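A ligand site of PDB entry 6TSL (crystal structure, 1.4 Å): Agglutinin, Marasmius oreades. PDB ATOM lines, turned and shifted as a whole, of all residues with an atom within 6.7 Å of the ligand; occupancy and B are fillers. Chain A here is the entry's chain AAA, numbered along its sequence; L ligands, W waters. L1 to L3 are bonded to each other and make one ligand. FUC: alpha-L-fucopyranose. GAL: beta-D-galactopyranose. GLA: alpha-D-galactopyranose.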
ATOM      1  N   HIS A   9       7.322  -6.298   4.070  1.00  0.00           N
ATOM      2  CA  HIS A   9       6.055  -6.845   4.572  1.00  0.00           C
ATOM      3  C   HIS A   9       5.968  -6.558   6.066  1.00  0.00           C
ATOM      4  O   HIS A   9       6.869  -6.979   6.780  1.00  0.00           O
ATOM      5  CB  HIS A   9       5.984  -8.331   4.257  1.00  0.00           C
ATOM      6  CG  HIS A   9       4.632  -8.928   4.450  1.00  0.00           C
ATOM      7  ND1 HIS A   9       4.379  -9.897   5.415  1.00  0.00           N
ATOM      8  CD2 HIS A   9       3.436  -8.664   3.859  1.00  0.00           C
ATOM      9  CE1 HIS A   9       3.095 -10.209   5.381  1.00  0.00           C
ATOM     10  NE2 HIS A   9       2.516  -9.488   4.409  1.00  0.00           N
ATOM     11  N   ASP A  20      -2.091  -3.624   5.370  1.00  0.00           N
ATOM     12  CA  ASP A  20      -2.752  -4.009   4.107  1.00  0.00           C
ATOM     13  C   ASP A  20      -3.491  -2.778   3.555  1.00  0.00           C
ATOM     14  O   ASP A  20      -4.258  -2.160   4.306  1.00  0.00           O
ATOM     15  CB  ASP A  20      -3.673  -5.198   4.333  1.00  0.00           C
ATOM     16  CG  ASP A  20      -4.353  -5.746   3.083  1.00  0.00           C
ATOM     17  OD1 ASP A  20      -5.183  -5.005   2.504  1.00  0.00           O
ATOM     18  OD2 ASP A  20      -4.190  -6.998   2.818  1.00  0.00           O
ATOM     19  N   LEU A  21      -3.230  -2.393   2.317  1.00  0.00           N
ATOM     20  CA  LEU A  21      -4.046  -1.351   1.642  1.00  0.00           C
ATOM     21  C   LEU A  21      -5.305  -2.016   1.085  1.00  0.00           C
ATOM     22  O   LEU A  21      -5.159  -2.885   0.183  1.00  0.00           O
ATOM     23  CB  LEU A  21      -3.231  -0.702   0.530  1.00  0.00           C
ATOM     24  CG  LEU A  21      -3.962   0.408  -0.227  1.00  0.00           C
ATOM     25  CD1 LEU A  21      -4.312   1.559   0.682  1.00  0.00           C
ATOM     26  CD2 LEU A  21      -3.119   0.908  -1.396  1.00  0.00           C
ATOM     27  N   LYS A  22      -6.468  -1.689   1.624  1.00  0.00           N
ATOM     28  CA  LYS A  22      -7.660  -2.535   1.420  1.00  0.00           C
ATOM     29  C   LYS A  22      -7.978  -2.629  -0.097  1.00  0.00           C
ATOM     30  O   LYS A  22      -8.150  -1.567  -0.751  1.00  0.00           O
ATOM     31  CB  LYS A  22      -8.860  -1.988   2.199  1.00  0.00           C
ATOM     32  CG  LYS A  22      -9.898  -3.027   2.503  1.00  0.00           C
ATOM     33  CD  LYS A  22     -11.030  -2.553   3.328  1.00  0.00           C
ATOM     34  CE  LYS A  22     -12.095  -3.626   3.501  1.00  0.00           C
ATOM     35  NZ  LYS A  22     -13.024  -3.291   4.610  1.00  0.00           N
ATOM     36  N   ASP A  23      -8.102  -3.851  -0.596  1.00  0.00           N
ATOM     37  CA  ASP A  23      -8.424  -4.185  -2.003  1.00  0.00           C
ATOM     38  C   ASP A  23      -7.342  -3.610  -2.950  1.00  0.00           C
ATOM     39  O   ASP A  23      -7.566  -3.612  -4.166  1.00  0.00           O
ATOM     40  CB  ASP A  23      -9.804  -3.665  -2.399  1.00  0.00           C
ATOM     41  CG  ASP A  23     -10.435  -4.458  -3.537  1.00  0.00           C
ATOM     42  OD1 ASP A  23     -10.187  -5.681  -3.607  1.00  0.00           O
ATOM     43  OD2 ASP A  23     -11.082  -3.834  -4.404  1.00  0.00           O
ATOM     44  N   GLY A  24      -6.213  -3.178  -2.407  1.00  0.00           N
ATOM     45  CA  GLY A  24      -5.121  -2.621  -3.218  1.00  0.00           C
ATOM     46  C   GLY A  24      -5.544  -1.331  -3.950  1.00  0.00           C
ATOM     47  O   GLY A  24      -4.878  -0.976  -4.927  1.00  0.00           O
ATOM     48  N   VAL A  33      -5.403  -1.301   6.748  1.00  0.00           N
ATOM     49  CA  VAL A  33      -6.049  -2.176   7.764  1.00  0.00           C
ATOM     50  C   VAL A  33      -5.093  -3.319   8.111  1.00  0.00           C
ATOM     51  O   VAL A  33      -4.201  -3.644   7.282  1.00  0.00           O
ATOM     52  CB  VAL A  33      -7.399  -2.719   7.238  1.00  0.00           C
ATOM     53  CG1 VAL A  33      -8.410  -1.601   7.042  1.00  0.00           C
ATOM     54  CG2 VAL A  33      -7.230  -3.519   5.952  1.00  0.00           C
ATOM     55  N   TRP A  35      -4.582  -7.348   8.241  1.00  0.00           N
ATOM     56  CA  TRP A  35      -5.093  -8.488   7.425  1.00  0.00           C
ATOM     57  C   TRP A  35      -4.144  -9.653   7.554  1.00  0.00           C
ATOM     58  O   TRP A  35      -2.933  -9.419   7.580  1.00  0.00           O
ATOM     59  CB  TRP A  35      -5.274  -8.066   5.948  1.00  0.00           C
ATOM     60  CG  TRP A  35      -6.337  -8.835   5.220  1.00  0.00           C
ATOM     61  CD1 TRP A  35      -6.249 -10.107   4.721  1.00  0.00           C
ATOM     62  CD2 TRP A  35      -7.676  -8.381   4.937  1.00  0.00           C
ATOM     63  NE1 TRP A  35      -7.455 -10.477   4.170  1.00  0.00           N
ATOM     64  CE2 TRP A  35      -8.336  -9.443   4.282  1.00  0.00           C
ATOM     65  CE3 TRP A  35      -8.381  -7.199   5.206  1.00  0.00           C
ATOM     66  CZ2 TRP A  35      -9.673  -9.331   3.871  1.00  0.00           C
ATOM     67  CZ3 TRP A  35      -9.688  -7.095   4.802  1.00  0.00           C
ATOM     68  CH2 TRP A  35     -10.327  -8.145   4.141  1.00  0.00           C
ATOM     69  N   GLN A  36      -4.655 -10.856   7.539  1.00  0.00           N
ATOM     70  CA  GLN A  36      -3.820 -12.063   7.641  1.00  0.00           C
ATOM     71  C   GLN A  36      -3.033 -12.252   6.335  1.00  0.00           C
ATOM     72  O   GLN A  36      -3.382 -11.600   5.335  1.00  0.00           O
ATOM     73  CB  GLN A  36      -4.687 -13.306   7.962  1.00  0.00           C
ATOM     74  CG  GLN A  36      -5.654 -13.708   6.861  1.00  0.00           C
ATOM     75  CD  GLN A  36      -6.437 -14.954   7.223  1.00  0.00           C
ATOM     76  OE1 GLN A  36      -5.869 -16.034   7.396  1.00  0.00           O
ATOM     77  NE2 GLN A  36      -7.729 -14.802   7.420  1.00  0.00           N
ATOM     78  N   PHE A  37      -2.029 -13.091   6.359  1.00  0.00           N
ATOM     79  CA  PHE A  37      -1.092 -13.225   5.224  1.00  0.00           C
ATOM     80  C   PHE A  37      -0.627 -14.659   5.110  1.00  0.00           C
ATOM     81  O   PHE A  37      -0.865 -15.456   6.030  1.00  0.00           O
ATOM     82  CB  PHE A  37       0.081 -12.259   5.415  1.00  0.00           C
ATOM     83  CG  PHE A  37       0.853 -12.426   6.697  1.00  0.00           C
ATOM     84  CD1 PHE A  37       1.970 -13.245   6.758  1.00  0.00           C
ATOM     85  CD2 PHE A  37       0.540 -11.672   7.825  1.00  0.00           C
ATOM     86  CE1 PHE A  37       2.701 -13.356   7.929  1.00  0.00           C
ATOM     87  CE2 PHE A  37       1.293 -11.761   8.981  1.00  0.00           C
ATOM     88  CZ  PHE A  37       2.343 -12.637   9.046  1.00  0.00           C
ATOM     89  N   THR A  38      -0.119 -15.003   3.952  1.00  0.00           N
ATOM     90  CA  THR A  38       0.467 -16.327   3.674  1.00  0.00           C
ATOM     91  C   THR A  38       1.951 -16.149   3.445  1.00  0.00           C
ATOM     92  O   THR A  38       2.350 -15.518   2.479  1.00  0.00           O
ATOM     93  CB  THR A  38      -0.211 -16.994   2.464  1.00  0.00           C
ATOM     94  OG1 THR A  38      -1.642 -16.866   2.607  1.00  0.00           O
ATOM     95  CG2 THR A  38       0.170 -18.446   2.320  1.00  0.00           C
ATOM     96  N   PRO A  39       2.808 -16.663   4.342  1.00  0.00           N
ATOM     97  CA  PRO A  39       4.258 -16.650   4.103  1.00  0.00           C
ATOM     98  C   PRO A  39       4.653 -17.338   2.780  1.00  0.00           C
ATOM     99  O   PRO A  39       3.899 -18.207   2.310  1.00  0.00           O
ATOM    100  CB  PRO A  39       4.834 -17.409   5.321  1.00  0.00           C
ATOM    101  CG  PRO A  39       3.810 -17.153   6.426  1.00  0.00           C
ATOM    102  CD  PRO A  39       2.470 -17.105   5.705  1.00  0.00           C
ATOM    103  N   THR A  41       4.566 -16.319  -0.230  1.00  0.00           N
ATOM    104  CA  THR A  41       3.779 -15.871  -1.389  1.00  0.00           C
ATOM    105  C   THR A  41       4.094 -14.418  -1.644  1.00  0.00           C
ATOM    106  O   THR A  41       4.602 -13.759  -0.712  1.00  0.00           O
ATOM    107  CB  THR A  41       2.255 -16.062  -1.160  1.00  0.00           C
ATOM    108  OG1 THR A  41       1.799 -15.092  -0.207  1.00  0.00           O
ATOM    109  CG2 THR A  41       1.892 -17.438  -0.690  1.00  0.00           C
ATOM    110  N   ILE A  42       3.618 -13.900  -2.749  1.00  0.00           N
ATOM    111  CA  ILE A  42       3.407 -12.455  -2.924  1.00  0.00           C
ATOM    112  C   ILE A  42       2.099 -12.069  -2.234  1.00  0.00           C
ATOM    113  O   ILE A  42       1.033 -12.595  -2.661  1.00  0.00           O
ATOM    114  CB  ILE A  42       3.399 -12.087  -4.412  1.00  0.00           C
ATOM    115  CG1 ILE A  42       4.746 -12.409  -5.071  1.00  0.00           C
ATOM    116  CG2 ILE A  42       3.012 -10.628  -4.588  1.00  0.00           C
ATOM    117  CD1 ILE A  42       5.915 -11.691  -4.463  1.00  0.00           C
ATOM    118  N   ASN A  43       2.182 -11.308  -1.165  1.00  0.00           N
ATOM    119  CA  ASN A  43       0.985 -10.711  -0.508  1.00  0.00           C
ATOM    120  C   ASN A  43       0.675  -9.370  -1.171  1.00  0.00           C
ATOM    121  O   ASN A  43       1.322  -8.362  -0.828  1.00  0.00           O
ATOM    122  CB  ASN A  43       1.179 -10.609   1.010  1.00  0.00           C
ATOM    123  CG  ASN A  43       1.208 -11.966   1.688  1.00  0.00           C
ATOM    124  OD1 ASN A  43       0.173 -12.604   1.864  1.00  0.00           O
ATOM    125  ND2 ASN A  43       2.410 -12.474   1.959  1.00  0.00           N
ATOM    126  N   TRP A  44      -0.182  -9.400  -2.189  1.00  0.00           N
ATOM    127  CA  TRP A  44      -0.259  -8.382  -3.263  1.00  0.00           C
ATOM    128  C   TRP A  44      -0.516  -6.985  -2.668  1.00  0.00           C
ATOM    129  O   TRP A  44      -0.108  -6.028  -3.288  1.00  0.00           O
ATOM    130  CB  TRP A  44      -1.332  -8.773  -4.276  1.00  0.00           C
ATOM    131  CG  TRP A  44      -0.865  -9.773  -5.257  1.00  0.00           C
ATOM    132  CD1 TRP A  44      -1.017 -11.133  -5.199  1.00  0.00           C
ATOM    133  CD2 TRP A  44      -0.047  -9.506  -6.405  1.00  0.00           C
ATOM    134  NE1 TRP A  44      -0.358 -11.723  -6.242  1.00  0.00           N
ATOM    135  CE2 TRP A  44       0.208 -10.753  -7.008  1.00  0.00           C
ATOM    136  CE3 TRP A  44       0.476  -8.357  -6.974  1.00  0.00           C
ATOM    137  CZ2 TRP A  44       0.954 -10.854  -8.178  1.00  0.00           C
ATOM    138  CZ3 TRP A  44       1.208  -8.469  -8.127  1.00  0.00           C
ATOM    139  CH2 TRP A  44       1.474  -9.705  -8.697  1.00  0.00           C
ATOM    140  N   HIS A  45      -1.300  -6.898  -1.590  1.00  0.00           N
ATOM    141  CA  HIS A  45      -1.767  -5.581  -1.077  1.00  0.00           C
ATOM    142  C   HIS A  45      -0.945  -5.151   0.143  1.00  0.00           C
ATOM    143  O   HIS A  45      -1.270  -4.092   0.727  1.00  0.00           O
ATOM    144  CB  HIS A  45      -3.271  -5.619  -0.780  1.00  0.00           C
ATOM    145  CG  HIS A  45      -4.110  -6.020  -1.942  1.00  0.00           C
ATOM    146  ND1 HIS A  45      -5.412  -6.512  -1.787  1.00  0.00           N
ATOM    147  CD2 HIS A  45      -3.898  -5.932  -3.288  1.00  0.00           C
ATOM    148  CE1 HIS A  45      -5.933  -6.773  -2.995  1.00  0.00           C
ATOM    149  NE2 HIS A  45      -5.050  -6.417  -3.931  1.00  0.00           N
ATOM    150  N   GLN A  46       0.136  -5.861   0.444  1.00  0.00           N
ATOM    151  CA  GLN A  46       0.797  -5.786   1.785  1.00  0.00           C
ATOM    152  C   GLN A  46       2.306  -5.496   1.626  1.00  0.00           C
ATOM    153  O   GLN A  46       3.043  -5.769   2.580  1.00  0.00           O
ATOM    154  CB  GLN A  46       0.580  -7.075   2.559  1.00  0.00           C
ATOM    155  CG  GLN A  46      -0.885  -7.432   2.739  1.00  0.00           C
ATOM    156  CD  GLN A  46      -1.106  -8.681   3.554  1.00  0.00           C
ATOM    157  OE1 GLN A  46      -0.180  -9.455   3.837  1.00  0.00           O
ATOM    158  NE2 GLN A  46      -2.381  -8.949   3.852  1.00  0.00           N
ATOM    159  N   PHE A  66       1.700  -2.157  -4.963  1.00  0.00           N
ATOM    160  CA  PHE A  66       0.620  -2.508  -5.915  1.00  0.00           C
ATOM    161  C   PHE A  66      -0.067  -1.211  -6.412  1.00  0.00           C
ATOM    162  O   PHE A  66      -0.187  -1.022  -7.620  1.00  0.00           O
ATOM    163  CB  PHE A  66      -0.371  -3.459  -5.281  1.00  0.00           C
ATOM    164  CG  PHE A  66      -1.484  -3.893  -6.190  1.00  0.00           C
ATOM    165  CD1 PHE A  66      -1.273  -4.877  -7.150  1.00  0.00           C
ATOM    166  CD2 PHE A  66      -2.724  -3.296  -6.129  1.00  0.00           C
ATOM    167  CE1 PHE A  66      -2.304  -5.272  -7.988  1.00  0.00           C
ATOM    168  CE2 PHE A  66      -3.752  -3.691  -6.977  1.00  0.00           C
ATOM    169  CZ  PHE A  66      -3.528  -4.673  -7.903  1.00  0.00           C
ATOM    170  N   ASP A 131      -9.568  -9.648   9.959  1.00  0.00           N
ATOM    171  CA  ASP A 131      -9.285  -9.091   8.604  1.00  0.00           C
ATOM    172  C   ASP A 131     -10.068  -7.800   8.424  1.00  0.00           C
ATOM    173  O   ASP A 131     -11.300  -7.824   8.571  1.00  0.00           O
ATOM    174  CB  ASP A 131      -9.620 -10.107   7.524  1.00  0.00           C
ATOM    175  CG  ASP A 131      -8.692 -11.296   7.493  1.00  0.00           C
ATOM    176  OD1 ASP A 131      -7.544 -11.173   8.037  1.00  0.00           O
ATOM    177  OD2 ASP A 131      -9.097 -12.333   6.971  1.00  0.00           O
HETATM  178  C1  FUC L   1      -5.710 -12.278  -2.110  1.00  0.00           C
HETATM  179  C2  FUC L   1      -6.302 -13.555  -2.701  1.00  0.00           C
HETATM  180  C3  FUC L   1      -7.109 -13.250  -3.980  1.00  0.00           C
HETATM  181  C4  FUC L   1      -6.289 -12.428  -4.924  1.00  0.00           C
HETATM  182  C5  FUC L   1      -5.802 -11.161  -4.236  1.00  0.00           C
HETATM  183  C6  FUC L   1      -4.954 -10.316  -5.132  1.00  0.00           C
HETATM  184  O2  FUC L   1      -7.114 -14.174  -1.700  1.00  0.00           O
HETATM  185  O3  FUC L   1      -7.503 -14.488  -4.595  1.00  0.00           O
HETATM  186  O4  FUC L   1      -5.129 -13.188  -5.408  1.00  0.00           O
HETATM  187  O5  FUC L   1      -5.006 -11.528  -3.104  1.00  0.00           O
HETATM  188  C1  GAL L   2      -7.805  -9.404  -1.247  1.00  0.00           C
HETATM  189  C2  GAL L   2      -6.527 -10.226  -1.034  1.00  0.00           C
HETATM  190  C3  GAL L   2      -6.205 -10.383   0.439  1.00  0.00           C
HETATM  191  C4  GAL L   2      -6.213  -9.032   1.134  1.00  0.00           C
HETATM  192  C5  GAL L   2      -7.532  -8.304   0.828  1.00  0.00           C
HETATM  193  C6  GAL L   2      -7.657  -6.944   1.495  1.00  0.00           C
HETATM  194  O1  GAL L   2      -7.963  -9.190  -2.608  1.00  0.00           O
HETATM  195  O2  GAL L   2      -6.714 -11.514  -1.631  1.00  0.00           O
HETATM  196  O3  GAL L   2      -4.911 -11.084   0.575  1.00  0.00           O
HETATM  197  O4  GAL L   2      -5.092  -8.227   0.704  1.00  0.00           O
HETATM  198  O5  GAL L   2      -7.668  -8.149  -0.600  1.00  0.00           O
HETATM  199  O6  GAL L   2      -6.845  -5.960   0.818  1.00  0.00           O
HETATM  200  C1  GLA L   3      -4.452 -11.401   1.802  1.00  0.00           C
HETATM  201  C2  GLA L   3      -3.142 -12.223   1.795  1.00  0.00           C
HETATM  202  C3  GLA L   3      -3.420 -13.649   1.329  1.00  0.00           C
HETATM  203  C4  GLA L   3      -4.566 -14.231   2.158  1.00  0.00           C
HETATM  204  C5  GLA L   3      -5.785 -13.353   2.022  1.00  0.00           C
HETATM  205  C6  GLA L   3      -7.020 -13.894   2.779  1.00  0.00           C
HETATM  206  O2  GLA L   3      -2.190 -11.609   0.941  1.00  0.00           O
HETATM  207  O3  GLA L   3      -2.240 -14.431   1.457  1.00  0.00           O
HETATM  208  O4  GLA L   3      -4.155 -14.361   3.550  1.00  0.00           O
HETATM  209  O5  GLA L   3      -5.463 -12.072   2.538  1.00  0.00           O
HETATM  210  O6  GLA L   3      -8.188 -13.010   2.603  1.00  0.00           O
HETATM  211  O   HOH W   1      -2.550  -9.020  -0.015  1.00  0.00           O
HETATM  212  O   HOH W   2     -10.162 -12.807   4.458  1.00  0.00           O
HETATM  213  O   HOH W   3      -9.075 -13.007  -0.025  1.00  0.00           O
HETATM  214  O   HOH W   4      -5.845 -16.121  -0.271  1.00  0.00           O
HETATM  215  O   HOH W   5      -2.974 -13.985  -3.782  1.00  0.00           O
HETATM  216  O   HOH W   6      -0.789 -14.215  -0.794  1.00  0.00           O
HETATM  217  O   HOH W   7      -2.090 -11.877  -1.989  1.00  0.00           O
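Merely in contact with the ligand: Leu 21, Lys 22, Phe 37 and Gln 46. Hydrophobic or aromatic side chains that line the ligand: Trp 35 and His 45. 11 residues have an atom within 4 Å of the ligand: Asp 20, Leu 21, Lys 22, Asp 23, Trp 35, Gln 36, Phe 37, Thr 38, Asn 43, His 45 and Gln 46.
OE1 of Gln 46 is in hydrogen-bond range of NE2 of His 9 (2.8 Å). NE2 of Gln 36 is in hydrogen-bond range of OD2 of Asp 131, at 2.9 Å. The backbone NH (N) of Val 33 lies within hydrogen-bond range of the backbone carbonyl oxygen (O) of Asp 20 (2.8 Å). NE2 of Gln 46 is in hydrogen-bond range of O of Gln 36 (3.2 Å). A ring nitrogen (ND1) of His 45 is in hydrogen-bond range of the backbone NH of Gly 24, at 3.5 Å. The side-chain carboxylate of Asp 20 lies within hydrogen-bond range of the side-chain amide nitrogen of Gln 46 (2.9 Å). The backbone carbonyl oxygen of Thr 38 is in hydrogen-bond range of the side-chain hydroxyl of Thr 41, at 2.8 Å. N of Leu 21 sits at hydrogen-bond distance from O of His 45, 3.0 Å away.
Water W6 lies within hydrogen-bond range of O3 of GLA L3, OG1 of Thr 41, O of Ile 42 and OD1 of Asn 43. Water W2 bridges an oxygen (O6) of GLA L3 and the side-chain carboxylate of Asp 131. Water W1 lies within hydrogen-bond range of an oxygen (O4) of GAL L2 (2.8 Å), the backbone NH of His 45 (2.9 Å) and the backbone NH of Trp 44 (3.2 Å). Water W7 lies within hydrogen-bond range of O2 of GLA L3, N of Trp 44 and O of Ile 42.
O2 of GLA L3 is in hydrogen-bond range of OD1 of Asn 43 (2.7 Å). The indole nitrogen (NE1) of Trp 35 is in hydrogen-bond range of an oxygen (O5) of GLA L3, 3.0 Å away. O6 of GAL L2 sits at hydrogen-bond distance from N of Asp 23 (2.8 Å). The side-chain carboxylate (OD1) of Asp 20 sits at hydrogen-bond distance from an oxygen (O6) of GAL L2 (2.6 Å). OG1 of Thr 38 sits at hydrogen-bond distance from O3 of GLA L3, 2.8 Å away. O3 of GLA L3 lies within hydrogen-bond range of N of Thr 38 (3.3 Å). The backbone carbonyl oxygen of Gln 36 lies within hydrogen-bond range of an oxygen (O4) of GLA L3 (3.4 Å). An oxygen (O6) of GAL L2 is in hydrogen-bond range of a ring nitrogen (ND1) of His 45, 3.0 Å away.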
